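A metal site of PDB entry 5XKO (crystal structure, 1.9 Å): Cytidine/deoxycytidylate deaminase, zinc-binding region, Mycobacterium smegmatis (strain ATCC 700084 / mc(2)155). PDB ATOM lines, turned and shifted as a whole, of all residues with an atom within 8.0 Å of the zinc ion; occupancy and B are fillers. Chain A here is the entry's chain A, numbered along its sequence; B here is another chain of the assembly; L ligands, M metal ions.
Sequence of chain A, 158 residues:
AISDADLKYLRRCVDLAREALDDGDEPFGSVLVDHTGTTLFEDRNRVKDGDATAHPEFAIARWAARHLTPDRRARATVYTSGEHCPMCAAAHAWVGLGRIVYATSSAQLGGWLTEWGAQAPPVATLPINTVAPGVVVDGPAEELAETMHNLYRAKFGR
O of Ala 52 sits at hydrogen-bond distance from NE2 of His 55 (2.9 Å). The side-chain sulfur (SG) of Cys 88 lies close to the backbone NH (N) of Phe 58. The backbone NH (N) of Met 87 lies close to the side-chain sulfur (SG) of Cys 85 (3.4 Å). SG of Cys 85 sits close to NE1 of Trp 94 of chain B, 3.5 Å away.
Within 4 Å of the zinc ion: His 55, Cys 85 and Cys 88. The nearest printed residue that does not touch the zinc ion is Met 87 (4.2 Å).
The zinc ion is bound by O1 of the ligand, 1.9 Å away. The zinc ion is bound by ND1 of His 55, 2.1 Å away. The side-chain sulfur (SG) of Cys 88 is bound to the zinc ion (2.3 Å). The zinc ion is bound by SG of Cys 85 (2.3 Å).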
ATOM      1  N   PHE A  28      21.953  21.656  -9.558  1.00  0.00           N
ATOM      2  CA  PHE A  28      22.991  21.641  -8.488  1.00  0.00           C
ATOM      3  C   PHE A  28      23.223  20.236  -8.017  1.00  0.00           C
ATOM      4  O   PHE A  28      22.269  19.523  -7.642  1.00  0.00           O
ATOM      5  CB  PHE A  28      22.590  22.567  -7.328  1.00  0.00           C
ATOM      6  CG  PHE A  28      22.384  23.965  -7.722  1.00  0.00           C
ATOM      7  CD1 PHE A  28      23.447  24.826  -7.887  1.00  0.00           C
ATOM      8  CD2 PHE A  28      21.122  24.452  -7.948  1.00  0.00           C
ATOM      9  CE1 PHE A  28      23.253  26.126  -8.293  1.00  0.00           C
ATOM     10  CE2 PHE A  28      20.944  25.779  -8.344  1.00  0.00           C
ATOM     11  CZ  PHE A  28      21.979  26.640  -8.504  1.00  0.00           C
ATOM     12  N   ASN A  45      19.876  18.884  -6.048  1.00  0.00           N
ATOM     13  CA  ASN A  45      18.786  19.774  -5.674  1.00  0.00           C
ATOM     14  C   ASN A  45      17.404  19.034  -5.801  1.00  0.00           C
ATOM     15  O   ASN A  45      17.230  18.234  -6.723  1.00  0.00           O
ATOM     16  CB  ASN A  45      18.787  20.961  -6.570  1.00  0.00           C
ATOM     17  CG  ASN A  45      17.584  21.840  -6.351  1.00  0.00           C
ATOM     18  OD1 ASN A  45      16.470  21.602  -6.863  1.00  0.00           O
ATOM     19  ND2 ASN A  45      17.789  22.861  -5.526  1.00  0.00           N
ATOM     20  N   ALA A  52      12.460  25.375  -1.007  1.00  0.00           N
ATOM     21  CA  ALA A  52      13.617  26.031  -1.624  1.00  0.00           C
ATOM     22  C   ALA A  52      14.959  25.746  -0.893  1.00  0.00           C
ATOM     23  O   ALA A  52      16.012  26.020  -1.488  1.00  0.00           O
ATOM     24  CB  ALA A  52      13.403  27.518  -1.734  1.00  0.00           C
ATOM     25  N   THR A  53      14.935  25.199   0.321  1.00  0.00           N
ATOM     26  CA  THR A  53      16.176  24.899   1.006  1.00  0.00           C
ATOM     27  C   THR A  53      16.722  23.485   0.732  1.00  0.00           C
ATOM     28  O   THR A  53      17.708  23.082   1.317  1.00  0.00           O
ATOM     29  CB  THR A  53      16.028  25.068   2.521  1.00  0.00           C
ATOM     30  OG1 THR A  53      15.190  24.060   3.063  1.00  0.00           O
ATOM     31  CG2 THR A  53      15.514  26.442   2.907  1.00  0.00           C
ATOM     32  N   ALA A  54      16.096  22.750  -0.201  1.00  0.00           N
ATOM     33  CA  ALA A  54      16.520  21.369  -0.563  1.00  0.00           C
ATOM     34  C   ALA A  54      17.816  21.329  -1.390  1.00  0.00           C
ATOM     35  O   ALA A  54      17.872  20.820  -2.556  1.00  0.00           O
ATOM     36  CB  ALA A  54      15.359  20.670  -1.313  1.00  0.00           C
ATOM     37  N   HIS A  55      18.871  21.993  -0.849  1.00  0.00           N
ATOM     38  CA  HIS A  55      20.131  22.061  -1.517  1.00  0.00           C
ATOM     39  C   HIS A  55      20.965  20.845  -1.157  1.00  0.00           C
ATOM     40  O   HIS A  55      21.050  20.412   0.009  1.00  0.00           O
ATOM     41  CB  HIS A  55      20.898  23.323  -1.046  1.00  0.00           C
ATOM     42  CG  HIS A  55      20.208  24.591  -1.404  1.00  0.00           C
ATOM     43  ND1 HIS A  55      20.851  25.804  -1.376  1.00  0.00           N
ATOM     44  CD2 HIS A  55      18.928  24.856  -1.760  1.00  0.00           C
ATOM     45  CE1 HIS A  55      20.019  26.758  -1.740  1.00  0.00           C
ATOM     46  NE2 HIS A  55      18.838  26.206  -1.975  1.00  0.00           N
ATOM     47  N   PRO A  56      21.728  20.348  -2.164  1.00  0.00           N
ATOM     48  CA  PRO A  56      22.468  19.093  -1.894  1.00  0.00           C
ATOM     49  C   PRO A  56      23.613  19.279  -0.884  1.00  0.00           C
ATOM     50  O   PRO A  56      23.904  18.352  -0.153  1.00  0.00           O
ATOM     51  CB  PRO A  56      23.024  18.712  -3.252  1.00  0.00           C
ATOM     52  CG  PRO A  56      23.112  19.964  -4.024  1.00  0.00           C
ATOM     53  CD  PRO A  56      21.922  20.834  -3.554  1.00  0.00           C
ATOM     54  N   GLU A  57      24.249  20.452  -0.888  1.00  0.00           N
ATOM     55  CA  GLU A  57      25.353  20.661   0.040  1.00  0.00           C
ATOM     56  C   GLU A  57      24.839  20.642   1.486  1.00  0.00           C
ATOM     57  O   GLU A  57      25.552  20.202   2.416  1.00  0.00           O
ATOM     58  CB  GLU A  57      26.050  21.950  -0.259  1.00  0.00           C
ATOM     59  CG  GLU A  57      26.630  22.081  -1.624  1.00  0.00           C
ATOM     60  CD  GLU A  57      25.686  22.648  -2.709  1.00  0.00           C
ATOM     61  OE1 GLU A  57      24.402  22.639  -2.540  1.00  0.00           O
ATOM     62  OE2 GLU A  57      26.229  23.114  -3.761  1.00  0.00           O
ATOM     63  N   PHE A  58      23.649  21.188   1.681  1.00  0.00           N
ATOM     64  CA  PHE A  58      23.070  21.169   2.996  1.00  0.00           C
ATOM     65  C   PHE A  58      22.745  19.734   3.433  1.00  0.00           C
ATOM     66  O   PHE A  58      22.999  19.329   4.626  1.00  0.00           O
ATOM     67  CB  PHE A  58      21.801  22.002   3.037  1.00  0.00           C
ATOM     68  CG  PHE A  58      21.264  22.132   4.410  1.00  0.00           C
ATOM     69  CD1 PHE A  58      21.753  23.106   5.266  1.00  0.00           C
ATOM     70  CD2 PHE A  58      20.313  21.252   4.911  1.00  0.00           C
ATOM     71  CE1 PHE A  58      21.360  23.210   6.561  1.00  0.00           C
ATOM     72  CE2 PHE A  58      19.880  21.385   6.215  1.00  0.00           C
ATOM     73  CZ  PHE A  58      20.434  22.345   7.039  1.00  0.00           C
ATOM     74  N   GLY A  82      28.211  23.951  -8.160  1.00  0.00           N
ATOM     75  CA  GLY A  82      28.048  25.394  -7.957  1.00  0.00           C
ATOM     76  C   GLY A  82      28.544  25.694  -6.555  1.00  0.00           C
ATOM     77  O   GLY A  82      28.147  25.010  -5.587  1.00  0.00           O
ATOM     78  N   GLU A  83      29.348  26.716  -6.438  1.00  0.00           N
ATOM     79  CA  GLU A  83      29.786  27.201  -5.101  1.00  0.00           C
ATOM     80  C   GLU A  83      28.583  27.359  -4.115  1.00  0.00           C
ATOM     81  O   GLU A  83      27.633  28.053  -4.383  1.00  0.00           O
ATOM     82  CB  GLU A  83      30.498  28.557  -5.273  1.00  0.00           C
ATOM     83  CG  GLU A  83      30.941  29.194  -3.963  1.00  0.00           C
ATOM     84  CD  GLU A  83      31.722  30.510  -4.110  1.00  0.00           C
ATOM     85  OE1 GLU A  83      31.612  31.163  -5.191  1.00  0.00           O
ATOM     86  OE2 GLU A  83      32.358  30.895  -3.079  1.00  0.00           O
ATOM     87  N   HIS A  84      28.733  26.788  -2.932  1.00  0.00           N
ATOM     88  CA  HIS A  84      27.736  26.852  -1.856  1.00  0.00           C
ATOM     89  C   HIS A  84      27.177  28.256  -1.704  1.00  0.00           C
ATOM     90  O   HIS A  84      27.947  29.221  -1.485  1.00  0.00           O
ATOM     91  CB  HIS A  84      28.371  26.513  -0.496  1.00  0.00           C
ATOM     92  CG  HIS A  84      28.899  25.149  -0.365  1.00  0.00           C
ATOM     93  ND1 HIS A  84      29.653  24.507  -1.332  1.00  0.00           N
ATOM     94  CD2 HIS A  84      28.839  24.278   0.662  1.00  0.00           C
ATOM     95  CE1 HIS A  84      30.018  23.307  -0.904  1.00  0.00           C
ATOM     96  NE2 HIS A  84      29.456  23.114   0.269  1.00  0.00           N
ATOM     97  N   CYS A  85      25.875  28.387  -1.662  1.00  0.00           N
ATOM     98  CA  CYS A  85      25.202  29.565  -1.085  1.00  0.00           C
ATOM     99  C   CYS A  85      25.525  29.706   0.413  1.00  0.00           C
ATOM    100  O   CYS A  85      26.003  28.777   1.020  1.00  0.00           O
ATOM    101  CB  CYS A  85      23.701  29.509  -1.271  1.00  0.00           C
ATOM    102  SG  CYS A  85      22.748  28.497  -0.080  1.00  0.00           S
ATOM    103  N   PRO A  86      25.184  30.858   1.004  1.00  0.00           N
ATOM    104  CA  PRO A  86      25.532  31.065   2.391  1.00  0.00           C
ATOM    105  C   PRO A  86      24.876  30.100   3.334  1.00  0.00           C
ATOM    106  O   PRO A  86      25.482  29.749   4.352  1.00  0.00           O
ATOM    107  CB  PRO A  86      25.052  32.479   2.633  1.00  0.00           C
ATOM    108  CG  PRO A  86      25.240  33.183   1.355  1.00  0.00           C
ATOM    109  CD  PRO A  86      24.953  32.142   0.297  1.00  0.00           C
ATOM    110  N   MET A  87      23.659  29.622   3.010  1.00  0.00           N
ATOM    111  CA  MET A  87      23.043  28.622   3.852  1.00  0.00           C
ATOM    112  C   MET A  87      23.946  27.374   3.984  1.00  0.00           C
ATOM    113  O   MET A  87      24.213  26.831   5.049  1.00  0.00           O
ATOM    114  CB  MET A  87      21.698  28.181   3.227  1.00  0.00           C
ATOM    115  CG  MET A  87      20.933  27.283   4.113  1.00  0.00           C
ATOM    116  SD  MET A  87      19.328  26.777   3.433  1.00  0.00           S
ATOM    117  CE  MET A  87      19.930  25.568   2.264  1.00  0.00           C
ATOM    118  N   CYS A  88      24.390  26.923   2.820  1.00  0.00           N
ATOM    119  CA  CYS A  88      25.151  25.691   2.743  1.00  0.00           C
ATOM    120  C   CYS A  88      26.614  25.822   3.207  1.00  0.00           C
ATOM    121  O   CYS A  88      27.137  24.874   3.786  1.00  0.00           O
ATOM    122  CB  CYS A  88      25.098  25.177   1.350  1.00  0.00           C
ATOM    123  SG  CYS A  88      23.446  24.684   0.781  1.00  0.00           S
ATOM    124  N   ALA A  89      27.225  26.989   2.962  1.00  0.00           N
ATOM    125  CA  ALA A  89      28.615  27.242   3.450  1.00  0.00           C
ATOM    126  C   ALA A  89      28.640  27.244   4.942  1.00  0.00           C
ATOM    127  O   ALA A  89      29.474  26.642   5.584  1.00  0.00           O
ATOM    128  CB  ALA A  89      29.127  28.525   2.815  1.00  0.00           C
ATOM    129  N   VAL A 123      18.911  35.758  -1.426  1.00  0.00           N
ATOM    130  CA  VAL A 123      20.098  35.497  -0.597  1.00  0.00           C
ATOM    131  C   VAL A 123      21.311  35.963  -1.413  1.00  0.00           C
ATOM    132  O   VAL A 123      21.450  35.679  -2.664  1.00  0.00           O
ATOM    133  CB  VAL A 123      20.212  33.997  -0.308  1.00  0.00           C
ATOM    134  CG1 VAL A 123      21.494  33.686   0.409  1.00  0.00           C
ATOM    135  CG2 VAL A 123      19.061  33.540   0.540  1.00  0.00           C
ATOM    136  N   ALA B  90      19.863  32.808   5.631  1.00  0.00           N
ATOM    137  CA  ALA B  90      19.676  32.375   4.247  1.00  0.00           C
ATOM    138  C   ALA B  90      18.438  31.499   4.093  1.00  0.00           C
ATOM    139  O   ALA B  90      17.611  31.741   3.183  1.00  0.00           O
ATOM    140  CB  ALA B  90      20.874  31.640   3.768  1.00  0.00           C
ATOM    141  N   TRP B  94      15.319  32.172   1.635  1.00  0.00           N
ATOM    142  CA  TRP B  94      14.993  31.231   0.593  1.00  0.00           C
ATOM    143  C   TRP B  94      13.523  30.817   0.673  1.00  0.00           C
ATOM    144  O   TRP B  94      12.868  30.624  -0.357  1.00  0.00           O
ATOM    145  CB  TRP B  94      15.884  29.990   0.646  1.00  0.00           C
ATOM    146  CG  TRP B  94      17.289  30.094   0.161  1.00  0.00           C
ATOM    147  CD1 TRP B  94      18.420  29.588   0.813  1.00  0.00           C
ATOM    148  CD2 TRP B  94      17.747  30.621  -1.066  1.00  0.00           C
ATOM    149  NE1 TRP B  94      19.530  29.819   0.042  1.00  0.00           N
ATOM    150  CE2 TRP B  94      19.147  30.432  -1.120  1.00  0.00           C
ATOM    151  CE3 TRP B  94      17.100  31.195  -2.178  1.00  0.00           C
ATOM    152  CZ2 TRP B  94      19.893  30.830  -2.202  1.00  0.00           C
ATOM    153  CZ3 TRP B  94      17.866  31.615  -3.272  1.00  0.00           C
ATOM    154  CH2 TRP B  94      19.238  31.386  -3.274  1.00  0.00           C
HETATM  155 AS1  LIG L   1      23.643  25.839  -3.916  1.00  0.00          AS
HETATM  156  O1  LIG L   1      23.952  26.323  -2.273  1.00  0.00           O
HETATM  157  O2  LIG L   1      23.039  24.223  -3.969  1.00  0.00           O
HETATM  158  C1  LIG L   1      22.301  26.963  -4.649  1.00  0.00           C
HETATM  159  C2  LIG L   1      25.295  25.976  -4.948  1.00  0.00           C
HETATM  160 ZN    ZN M   1      22.814  26.266  -0.738  1.00  0.00          ZN
